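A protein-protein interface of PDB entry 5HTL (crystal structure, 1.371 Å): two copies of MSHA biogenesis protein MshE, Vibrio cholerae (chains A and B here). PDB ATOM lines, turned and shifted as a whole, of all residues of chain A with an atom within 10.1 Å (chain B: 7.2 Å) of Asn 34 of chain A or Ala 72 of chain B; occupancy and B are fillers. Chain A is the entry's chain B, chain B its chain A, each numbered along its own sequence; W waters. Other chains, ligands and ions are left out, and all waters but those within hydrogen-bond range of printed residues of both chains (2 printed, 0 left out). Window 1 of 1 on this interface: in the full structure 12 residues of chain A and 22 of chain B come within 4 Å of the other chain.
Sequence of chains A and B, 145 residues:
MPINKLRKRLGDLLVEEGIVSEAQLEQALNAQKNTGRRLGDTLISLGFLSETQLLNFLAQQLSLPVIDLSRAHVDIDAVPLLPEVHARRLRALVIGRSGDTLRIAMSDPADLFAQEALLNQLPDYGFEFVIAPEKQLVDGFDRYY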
ATOM      1  N   GLU A  26      -2.031  14.494 -14.629  1.00  0.00           N
ATOM      2  CA  GLU A  26      -1.895  13.312 -13.787  1.00  0.00           C
ATOM      3  C   GLU A  26      -2.932  13.286 -12.668  1.00  0.00           C
ATOM      4  O   GLU A  26      -3.522  12.244 -12.390  1.00  0.00           O
ATOM      5  CB  GLU A  26      -0.469  13.212 -13.236  1.00  0.00           C
ATOM      6  CG  GLU A  26       0.534  12.726 -14.278  1.00  0.00           C
ATOM      7  CD  GLU A  26       0.123  11.401 -14.906  1.00  0.00           C
ATOM      8  OE1 GLU A  26      -0.140  10.442 -14.151  1.00  0.00           O
ATOM      9  OE2 GLU A  26       0.054  11.322 -16.153  1.00  0.00           O
ATOM     10  N   GLN A  27      -3.177  14.431 -12.040  1.00  0.00           N
ATOM     11  CA  GLN A  27      -4.220  14.518 -11.023  1.00  0.00           C
ATOM     12  C   GLN A  27      -5.593  14.148 -11.586  1.00  0.00           C
ATOM     13  O   GLN A  27      -6.368  13.440 -10.945  1.00  0.00           O
ATOM     14  CB  GLN A  27      -4.259  15.920 -10.413  1.00  0.00           C
ATOM     15  CG  GLN A  27      -5.184  16.030  -9.212  1.00  0.00           C
ATOM     16  CD  GLN A  27      -5.164  17.410  -8.587  1.00  0.00           C
ATOM     17  OE1 GLN A  27      -4.268  18.203  -8.846  1.00  0.00           O
ATOM     18  NE2 GLN A  27      -6.157  17.699  -7.753  1.00  0.00           N
ATOM     19  N   ALA A  28      -5.889  14.630 -12.789  1.00  0.00           N
ATOM     20  CA  ALA A  28      -7.172  14.322 -13.404  1.00  0.00           C
ATOM     21  C   ALA A  28      -7.269  12.858 -13.796  1.00  0.00           C
ATOM     22  O   ALA A  28      -8.331  12.253 -13.648  1.00  0.00           O
ATOM     23  CB  ALA A  28      -7.423  15.217 -14.596  1.00  0.00           C
ATOM     24  N   LEU A  29      -6.187  12.279 -14.304  1.00  0.00           N
ATOM     25  CA  LEU A  29      -6.214  10.862 -14.674  1.00  0.00           C
ATOM     26  C   LEU A  29      -6.424   9.999 -13.446  1.00  0.00           C
ATOM     27  O   LEU A  29      -7.181   9.029 -13.485  1.00  0.00           O
ATOM     28  CB  LEU A  29      -4.940  10.461 -15.417  1.00  0.00           C
ATOM     29  CG  LEU A  29      -4.817  11.050 -16.821  1.00  0.00           C
ATOM     30  CD1 LEU A  29      -3.403  10.858 -17.361  1.00  0.00           C
ATOM     31  CD2 LEU A  29      -5.828  10.427 -17.763  1.00  0.00           C
ATOM     32  N   ASN A  30      -5.784  10.362 -12.336  1.00  0.00           N
ATOM     33  CA  ASN A  30      -6.001   9.636 -11.087  1.00  0.00           C
ATOM     34  C   ASN A  30      -7.438   9.775 -10.594  1.00  0.00           C
ATOM     35  O   ASN A  30      -8.053   8.811 -10.126  1.00  0.00           O
ATOM     36  CB  ASN A  30      -5.027  10.115 -10.004  1.00  0.00           C
ATOM     37  CG  ASN A  30      -3.585   9.740 -10.298  1.00  0.00           C
ATOM     38  OD1 ASN A  30      -2.655  10.374  -9.793  1.00  0.00           O
ATOM     39  ND2 ASN A  30      -3.387   8.710 -11.117  1.00  0.00           N
ATOM     40  N   ALA A  31      -7.989  10.975 -10.697  1.00  0.00           N
ATOM     41  CA  ALA A  31      -9.347  11.204 -10.238  1.00  0.00           C
ATOM     42  C   ALA A  31     -10.327  10.398 -11.076  1.00  0.00           C
ATOM     43  O   ALA A  31     -11.293   9.832 -10.556  1.00  0.00           O
ATOM     44  CB  ALA A  31      -9.680  12.687 -10.285  1.00  0.00           C
ATOM     45  N   GLN A  32     -10.062  10.339 -12.378  1.00  0.00           N
ATOM     46  CA  GLN A  32     -10.931   9.627 -13.307  1.00  0.00           C
ATOM     47  C   GLN A  32     -10.967   8.131 -13.016  1.00  0.00           C
ATOM     48  O   GLN A  32     -12.000   7.478 -13.196  1.00  0.00           O
ATOM     49  CB  GLN A  32     -10.457   9.852 -14.745  1.00  0.00           C
ATOM     50  CG  GLN A  32     -11.201   8.975 -15.767  1.00  0.00           C
ATOM     51  CD  GLN A  32     -10.738   9.210 -17.181  1.00  0.00           C
ATOM     52  OE1 GLN A  32      -9.582   8.940 -17.516  1.00  0.00           O
ATOM     53  NE2 GLN A  32     -11.632   9.706 -18.023  1.00  0.00           N
ATOM     54  N   LYS A  33      -9.842   7.578 -12.561  1.00  0.00           N
ATOM     55  CA  LYS A  33      -9.795   6.162 -12.205  1.00  0.00           C
ATOM     56  C   LYS A  33     -10.807   5.856 -11.106  1.00  0.00           C
ATOM     57  O   LYS A  33     -11.294   4.730 -10.985  1.00  0.00           O
ATOM     58  CB  LYS A  33      -8.390   5.786 -11.753  1.00  0.00           C
ATOM     59  CG  LYS A  33      -7.400   5.696 -12.887  1.00  0.00           C
ATOM     60  CD  LYS A  33      -5.983   5.734 -12.350  1.00  0.00           C
ATOM     61  CE  LYS A  33      -4.961   5.637 -13.473  1.00  0.00           C
ATOM     62  NZ  LYS A  33      -4.539   6.968 -13.991  1.00  0.00           N
ATOM     63  N   ASN A  34     -11.146   6.873 -10.318  1.00  0.00           N
ATOM     64  CA  ASN A  34     -12.118   6.709  -9.250  1.00  0.00           C
ATOM     65  C   ASN A  34     -13.537   7.189  -9.557  1.00  0.00           C
ATOM     66  O   ASN A  34     -14.379   7.204  -8.676  1.00  0.00           O
ATOM     67  CB  ASN A  34     -11.606   7.363  -7.961  1.00  0.00           C
ATOM     68  CG  ASN A  34     -10.364   6.685  -7.426  1.00  0.00           C
ATOM     69  OD1 ASN A  34     -10.216   5.469  -7.531  1.00  0.00           O
ATOM     70  ND2 ASN A  34      -9.452   7.474  -6.867  1.00  0.00           N
ATOM     71  N   THR A  35     -13.816   7.580 -10.798  1.00  0.00           N
ATOM     72  CA  THR A  35     -15.176   8.007 -11.135  1.00  0.00           C
ATOM     73  C   THR A  35     -15.660   7.433 -12.464  1.00  0.00           C
ATOM     74  O   THR A  35     -16.831   7.078 -12.611  1.00  0.00           O
ATOM     75  CB  THR A  35     -15.321   9.527 -11.241  1.00  0.00           C
ATOM     76  OG1 THR A  35     -14.545   9.993 -12.350  1.00  0.00           O
ATOM     77  CG2 THR A  35     -14.859  10.236  -9.978  1.00  0.00           C
ATOM     78  N   GLY A  36     -14.773   7.354 -13.448  1.00  0.00           N
ATOM     79  CA  GLY A  36     -15.196   6.979 -14.783  1.00  0.00           C
ATOM     80  C   GLY A  36     -15.770   8.123 -15.602  1.00  0.00           C
ATOM     81  O   GLY A  36     -16.180   7.894 -16.742  1.00  0.00           O
ATOM     82  N   ARG A  37     -15.799   9.332 -15.041  1.00  0.00           N
ATOM     83  CA  ARG A  37     -16.220  10.495 -15.821  1.00  0.00           C
ATOM     84  C   ARG A  37     -15.211  10.754 -16.929  1.00  0.00           C
ATOM     85  O   ARG A  37     -14.061  10.308 -16.847  1.00  0.00           O
ATOM     86  CB  ARG A  37     -16.361  11.727 -14.919  1.00  0.00           C
ATOM     87  CG  ARG A  37     -17.505  11.590 -13.895  1.00  0.00           C
ATOM     88  CD  ARG A  37     -17.673  12.842 -13.052  1.00  0.00           C
ATOM     89  NE  ARG A  37     -18.164  13.971 -13.840  1.00  0.00           N
ATOM     90  CZ  ARG A  37     -17.694  15.215 -13.754  1.00  0.00           C
ATOM     91  NH1 ARG A  37     -18.212  16.164 -14.506  1.00  0.00           N
ATOM     92  NH2 ARG A  37     -16.708  15.511 -12.917  1.00  0.00           N
ATOM     93  N   ARG A  38     -15.623  11.488 -17.957  1.00  0.00           N
ATOM     94  CA  ARG A  38     -14.697  11.847 -19.027  1.00  0.00           C
ATOM     95  C   ARG A  38     -13.546  12.703 -18.507  1.00  0.00           C
ATOM     96  O   ARG A  38     -13.689  13.427 -17.512  1.00  0.00           O
ATOM     97  CB  ARG A  38     -15.437  12.591 -20.131  1.00  0.00           C
ATOM     98  CG  ARG A  38     -16.532  11.778 -20.795  1.00  0.00           C
ATOM     99  CD  ARG A  38     -17.170  12.586 -21.909  1.00  0.00           C
ATOM    100  NE  ARG A  38     -18.325  11.935 -22.520  1.00  0.00           N
ATOM    101  CZ  ARG A  38     -19.567  12.036 -22.057  1.00  0.00           C
ATOM    102  NH1 ARG A  38     -19.811  12.750 -20.964  1.00  0.00           N
ATOM    103  NH2 ARG A  38     -20.564  11.414 -22.676  1.00  0.00           N
ATOM    104  N   THR A  42     -13.553  15.928 -15.970  1.00  0.00           N
ATOM    105  CA  THR A  42     -12.760  15.832 -14.744  1.00  0.00           C
ATOM    106  C   THR A  42     -11.856  17.055 -14.584  1.00  0.00           C
ATOM    107  O   THR A  42     -11.768  17.644 -13.502  1.00  0.00           O
ATOM    108  CB  THR A  42     -11.931  14.528 -14.738  1.00  0.00           C
ATOM    109  OG1 THR A  42     -12.809  13.403 -14.820  1.00  0.00           O
ATOM    110  CG2 THR A  42     -11.105  14.389 -13.470  1.00  0.00           C
ATOM    111  N   VAL B  66     -10.382   3.112 -17.871  1.00  0.00           N
ATOM    112  CA  VAL B  66     -10.303   2.050 -16.881  1.00  0.00           C
ATOM    113  C   VAL B  66     -10.624   2.661 -15.523  1.00  0.00           C
ATOM    114  O   VAL B  66     -10.114   3.738 -15.191  1.00  0.00           O
ATOM    115  CB  VAL B  66      -8.879   1.465 -16.812  1.00  0.00           C
ATOM    116  CG1 VAL B  66      -8.798   0.381 -15.761  1.00  0.00           C
ATOM    117  CG2 VAL B  66      -8.443   0.939 -18.164  1.00  0.00           C
ATOM    118  N   ILE B  67     -11.473   2.007 -14.740  1.00  0.00           N
ATOM    119  CA  ILE B  67     -11.683   2.458 -13.366  1.00  0.00           C
ATOM    120  C   ILE B  67     -11.167   1.442 -12.368  1.00  0.00           C
ATOM    121  O   ILE B  67     -11.081   0.245 -12.663  1.00  0.00           O
ATOM    122  CB  ILE B  67     -13.174   2.778 -13.051  1.00  0.00           C
ATOM    123  CG1 ILE B  67     -14.068   1.548 -13.226  1.00  0.00           C
ATOM    124  CG2 ILE B  67     -13.642   3.947 -13.917  1.00  0.00           C
ATOM    125  CD1 ILE B  67     -15.415   1.690 -12.540  1.00  0.00           C
ATOM    126  N   ASP B  68     -10.799   1.944 -11.196  1.00  0.00           N
ATOM    127  CA  ASP B  68     -10.524   1.083 -10.058  1.00  0.00           C
ATOM    128  C   ASP B  68     -11.821   0.961  -9.278  1.00  0.00           C
ATOM    129  O   ASP B  68     -12.126   1.791  -8.418  1.00  0.00           O
ATOM    130  CB  ASP B  68      -9.433   1.692  -9.181  1.00  0.00           C
ATOM    131  CG  ASP B  68      -9.095   0.828  -7.986  1.00  0.00           C
ATOM    132  OD1 ASP B  68      -9.761  -0.211  -7.768  1.00  0.00           O
ATOM    133  OD2 ASP B  68      -8.159   1.203  -7.246  1.00  0.00           O
ATOM    134  N   LEU B  69     -12.581  -0.083  -9.570  1.00  0.00           N
ATOM    135  CA  LEU B  69     -13.901  -0.236  -8.993  1.00  0.00           C
ATOM    136  C   LEU B  69     -13.858  -0.515  -7.476  1.00  0.00           C
ATOM    137  O   LEU B  69     -14.843  -0.313  -6.775  1.00  0.00           O
ATOM    138  CB  LEU B  69     -14.654  -1.316  -9.766  1.00  0.00           C
ATOM    139  CG  LEU B  69     -16.122  -1.542  -9.447  1.00  0.00           C
ATOM    140  CD1 LEU B  69     -16.925  -0.241  -9.507  1.00  0.00           C
ATOM    141  CD2 LEU B  69     -16.682  -2.578 -10.415  1.00  0.00           C
ATOM    142  N   SER B  70     -12.700  -0.932  -6.973  1.00  0.00           N
ATOM    143  CA  SER B  70     -12.541  -1.172  -5.538  1.00  0.00           C
ATOM    144  C   SER B  70     -12.532   0.136  -4.747  1.00  0.00           C
ATOM    145  O   SER B  70     -12.722   0.147  -3.529  1.00  0.00           O
ATOM    146  CB  SER B  70     -11.252  -1.940  -5.257  1.00  0.00           C
ATOM    147  OG  SER B  70     -10.119  -1.092  -5.323  1.00  0.00           O
ATOM    148  N   ARG B  71     -12.319   1.246  -5.442  1.00  0.00           N
ATOM    149  CA  ARG B  71     -12.211   2.536  -4.780  1.00  0.00           C
ATOM    150  C   ARG B  71     -13.113   3.572  -5.402  1.00  0.00           C
ATOM    151  O   ARG B  71     -13.260   4.672  -4.876  1.00  0.00           O
ATOM    152  CB  ARG B  71     -10.771   3.041  -4.844  1.00  0.00           C
ATOM    153  CG  ARG B  71      -9.895   2.488  -3.746  1.00  0.00           C
ATOM    154  CD  ARG B  71      -8.501   3.063  -3.822  1.00  0.00           C
ATOM    155  NE  ARG B  71      -8.158   3.852  -2.644  1.00  0.00           N
ATOM    156  CZ  ARG B  71      -7.454   4.976  -2.685  1.00  0.00           C
ATOM    157  NH1 ARG B  71      -7.029   5.449  -3.850  1.00  0.00           N
ATOM    158  NH2 ARG B  71      -7.182   5.635  -1.566  1.00  0.00           N
ATOM    159  N   ALA B  72     -13.697   3.230  -6.543  1.00  0.00           N
ATOM    160  CA  ALA B  72     -14.449   4.213  -7.307  1.00  0.00           C
ATOM    161  C   ALA B  72     -15.748   4.623  -6.624  1.00  0.00           C
ATOM    162  O   ALA B  72     -16.330   3.882  -5.832  1.00  0.00           O
ATOM    163  CB  ALA B  72     -14.723   3.702  -8.718  1.00  0.00           C
ATOM    164  N   HIS B  73     -16.184   5.839  -6.933  1.00  0.00           N
ATOM    165  CA  HIS B  73     -17.501   6.308  -6.558  1.00  0.00           C
ATOM    166  C   HIS B  73     -18.536   5.425  -7.233  1.00  0.00           C
ATOM    167  O   HIS B  73     -18.491   5.194  -8.445  1.00  0.00           O
ATOM    168  CB  HIS B  73     -17.686   7.759  -7.017  1.00  0.00           C
ATOM    169  CG  HIS B  73     -19.060   8.292  -6.769  1.00  0.00           C
ATOM    170  ND1 HIS B  73     -19.404   8.950  -5.609  1.00  0.00           N
ATOM    171  CD2 HIS B  73     -20.184   8.254  -7.527  1.00  0.00           C
ATOM    172  CE1 HIS B  73     -20.677   9.295  -5.663  1.00  0.00           C
ATOM    173  NE2 HIS B  73     -21.174   8.888  -6.815  1.00  0.00           N
ATOM    174  N   VAL B  74     -19.458   4.909  -6.436  1.00  0.00           N
ATOM    175  CA  VAL B  74     -20.571   4.150  -6.962  1.00  0.00           C
ATOM    176  C   VAL B  74     -21.829   4.674  -6.308  1.00  0.00           C
ATOM    177  O   VAL B  74     -21.914   4.751  -5.078  1.00  0.00           O
ATOM    178  CB  VAL B  74     -20.426   2.651  -6.665  1.00  0.00           C
ATOM    179  CG1 VAL B  74     -21.681   1.917  -7.088  1.00  0.00           C
ATOM    180  CG2 VAL B  74     -19.208   2.088  -7.386  1.00  0.00           C
ATOM    181  N   ASP B  75     -22.784   5.073  -7.134  1.00  0.00           N
ATOM    182  CA  ASP B  75     -24.090   5.451  -6.628  1.00  0.00           C
ATOM    183  C   ASP B  75     -24.838   4.172  -6.280  1.00  0.00           C
ATOM    184  O   ASP B  75     -25.440   3.538  -7.148  1.00  0.00           O
ATOM    185  CB  ASP B  75     -24.854   6.269  -7.671  1.00  0.00           C
ATOM    186  CG  ASP B  75     -26.181   6.809  -7.142  1.00  0.00           C
ATOM    187  OD1 ASP B  75     -26.591   6.428  -6.020  1.00  0.00           O
ATOM    188  OD2 ASP B  75     -26.818   7.613  -7.856  1.00  0.00           O
ATOM    189  N   ILE B  95     -23.141   2.089 -12.065  1.00  0.00           N
ATOM    190  CA  ILE B  95     -22.456   2.810 -10.990  1.00  0.00           C
ATOM    191  C   ILE B  95     -22.845   4.278 -10.902  1.00  0.00           C
ATOM    192  O   ILE B  95     -22.463   4.969  -9.962  1.00  0.00           O
ATOM    193  CB  ILE B  95     -20.909   2.689 -11.092  1.00  0.00           C
ATOM    194  CG1 ILE B  95     -20.387   3.343 -12.372  1.00  0.00           C
ATOM    195  CG2 ILE B  95     -20.478   1.221 -11.000  1.00  0.00           C
ATOM    196  CD1 ILE B  95     -18.843   3.437 -12.451  1.00  0.00           C
ATOM    197  N   ARG B 143     -20.924  -6.805  -3.056  1.00  0.00           N
ATOM    198  CA  ARG B 143     -20.895  -5.637  -2.189  1.00  0.00           C
ATOM    199  C   ARG B 143     -22.174  -4.809  -2.285  1.00  0.00           C
ATOM    200  O   ARG B 143     -22.686  -4.311  -1.272  1.00  0.00           O
ATOM    201  CB  ARG B 143     -19.686  -4.779  -2.592  1.00  0.00           C
ATOM    202  CG  ARG B 143     -19.476  -3.495  -1.829  1.00  0.00           C
ATOM    203  CD  ARG B 143     -18.025  -3.040  -1.958  1.00  0.00           C
ATOM    204  NE  ARG B 143     -17.752  -2.287  -3.186  1.00  0.00           N
ATOM    205  CZ  ARG B 143     -16.873  -2.645  -4.120  1.00  0.00           C
ATOM    206  NH1 ARG B 143     -16.170  -3.759  -3.990  1.00  0.00           N
ATOM    207  NH2 ARG B 143     -16.700  -1.887  -5.193  1.00  0.00           N
ATOM    208  N   TYR B 144     -22.696  -4.674  -3.502  1.00  0.00           N
ATOM    209  CA  TYR B 144     -23.776  -3.734  -3.769  1.00  0.00           C
ATOM    210  C   TYR B 144     -25.165  -4.357  -3.901  1.00  0.00           C
ATOM    211  O   TYR B 144     -26.163  -3.635  -3.919  1.00  0.00           O
ATOM    212  CB  TYR B 144     -23.460  -2.907  -5.013  1.00  0.00           C
ATOM    213  CG  TYR B 144     -22.225  -2.047  -4.862  1.00  0.00           C
ATOM    214  CD1 TYR B 144     -22.169  -1.043  -3.901  1.00  0.00           C
ATOM    215  CD2 TYR B 144     -21.112  -2.236  -5.672  1.00  0.00           C
ATOM    216  CE1 TYR B 144     -21.041  -0.253  -3.753  1.00  0.00           C
ATOM    217  CE2 TYR B 144     -19.981  -1.452  -5.529  1.00  0.00           C
ATOM    218  CZ  TYR B 144     -19.952  -0.463  -4.569  1.00  0.00           C
ATOM    219  OH  TYR B 144     -18.826   0.321  -4.429  1.00  0.00           O
HETATM  220  O   HOH W   1      -7.688   4.454  -7.605  1.00  0.00           O
HETATM  221  O   HOH W   2     -18.551   6.866 -10.453  1.00  0.00           O
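The backbone NH of Asp 68 of chain B is in hydrogen-bond range of the backbone carbonyl oxygen of Lys 33 of chain A (2.8 Å).
The backbone NH (N) of His 73 of chain B lies within hydrogen-bond range of the backbone carbonyl oxygen (O) of Asn 34 of chain A (2.9 Å).
Gln 32 of chain A touches Ile 67 of chain B.
Lys 33 of chain A touches Val 66 of chain B.
O of Lys 33 of chain A touches CA of Ile 67 of chain B, 3.3 Å away.
OD1 of Asn 34 of chain A touches CB of Arg 71 of chain B, 3.7 Å away.
O of Asn 34 of chain A touches CA of Ala 72 of chain B (3.3 Å).
CG2 of Ile 67 of chain B touches CA of Gly 36 of chain A, at 3.5 Å.
The side-chain carboxylate of Asp 68 of chain B is in hydrogen-bond range of the side-chain hydroxyl of Ser 70 of chain B (2.6 Å).
NZ of Lys 33 of chain A lies within hydrogen-bond range of O of Leu 29 of chain A, 3.4 Å away.
O of Arg 37 of chain A sits at hydrogen-bond distance from NE2 of Gln 32 of chain A, at 2.8 Å.
Of the 13 printed residues of chain B, 6 touch a printed residue of chain A.
Printed residues of chain B that touch a printed residue of chain A: Val 66, Ile 67, Asp 68, Arg 71, Ala 72 and His 73.
Hydrophobic or aromatic side chains of chain B that line the printed part of chain A: Ile 67, Ala 72 and His 73.
Printed residues of chain A that touch a printed residue of chain B: Gln 32, Lys 33, Asn 34 and Gly 36.
Among the printed residues, 8 pairs touch across the chains.
No position is printed for both chains.
Ala 72 of chain B touches just one residue of chain A: Asn 34.
Asp 68 of chain B touches just one residue of chain A: Lys 33 (2.8 Å).
No residue of chain A comes within 4 Å of Ser 70 of chain B.
No residue of chain A comes within 4 Å of Val 74 of chain B.
Printed residues of chain B within 4 Å of Lys 33 of chain A: Val 66 (3.9 Å), Ile 67 (3.3 Å) and Asp 68 (2.8 Å).
Printed residues of chain A within 4 Å of Arg 71 of chain B: Asn 34.
Glu 26 of chain A touches none of the printed residues of chain B.
The nearest printed residue of chain B that does not touch Lys 33 of chain A is Ala 72 of chain B (4.2 Å).
Water W2 lies within hydrogen-bond range of the backbone carbonyl oxygen of His 73 of chain B and the backbone carbonyl oxygen of Thr 35 of chain A.
Water W1 bridges the side-chain amide oxygen (OD1) of Asn 34 of chain A and the side-chain carboxylate (OD2) of Asp 68 of chain B.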
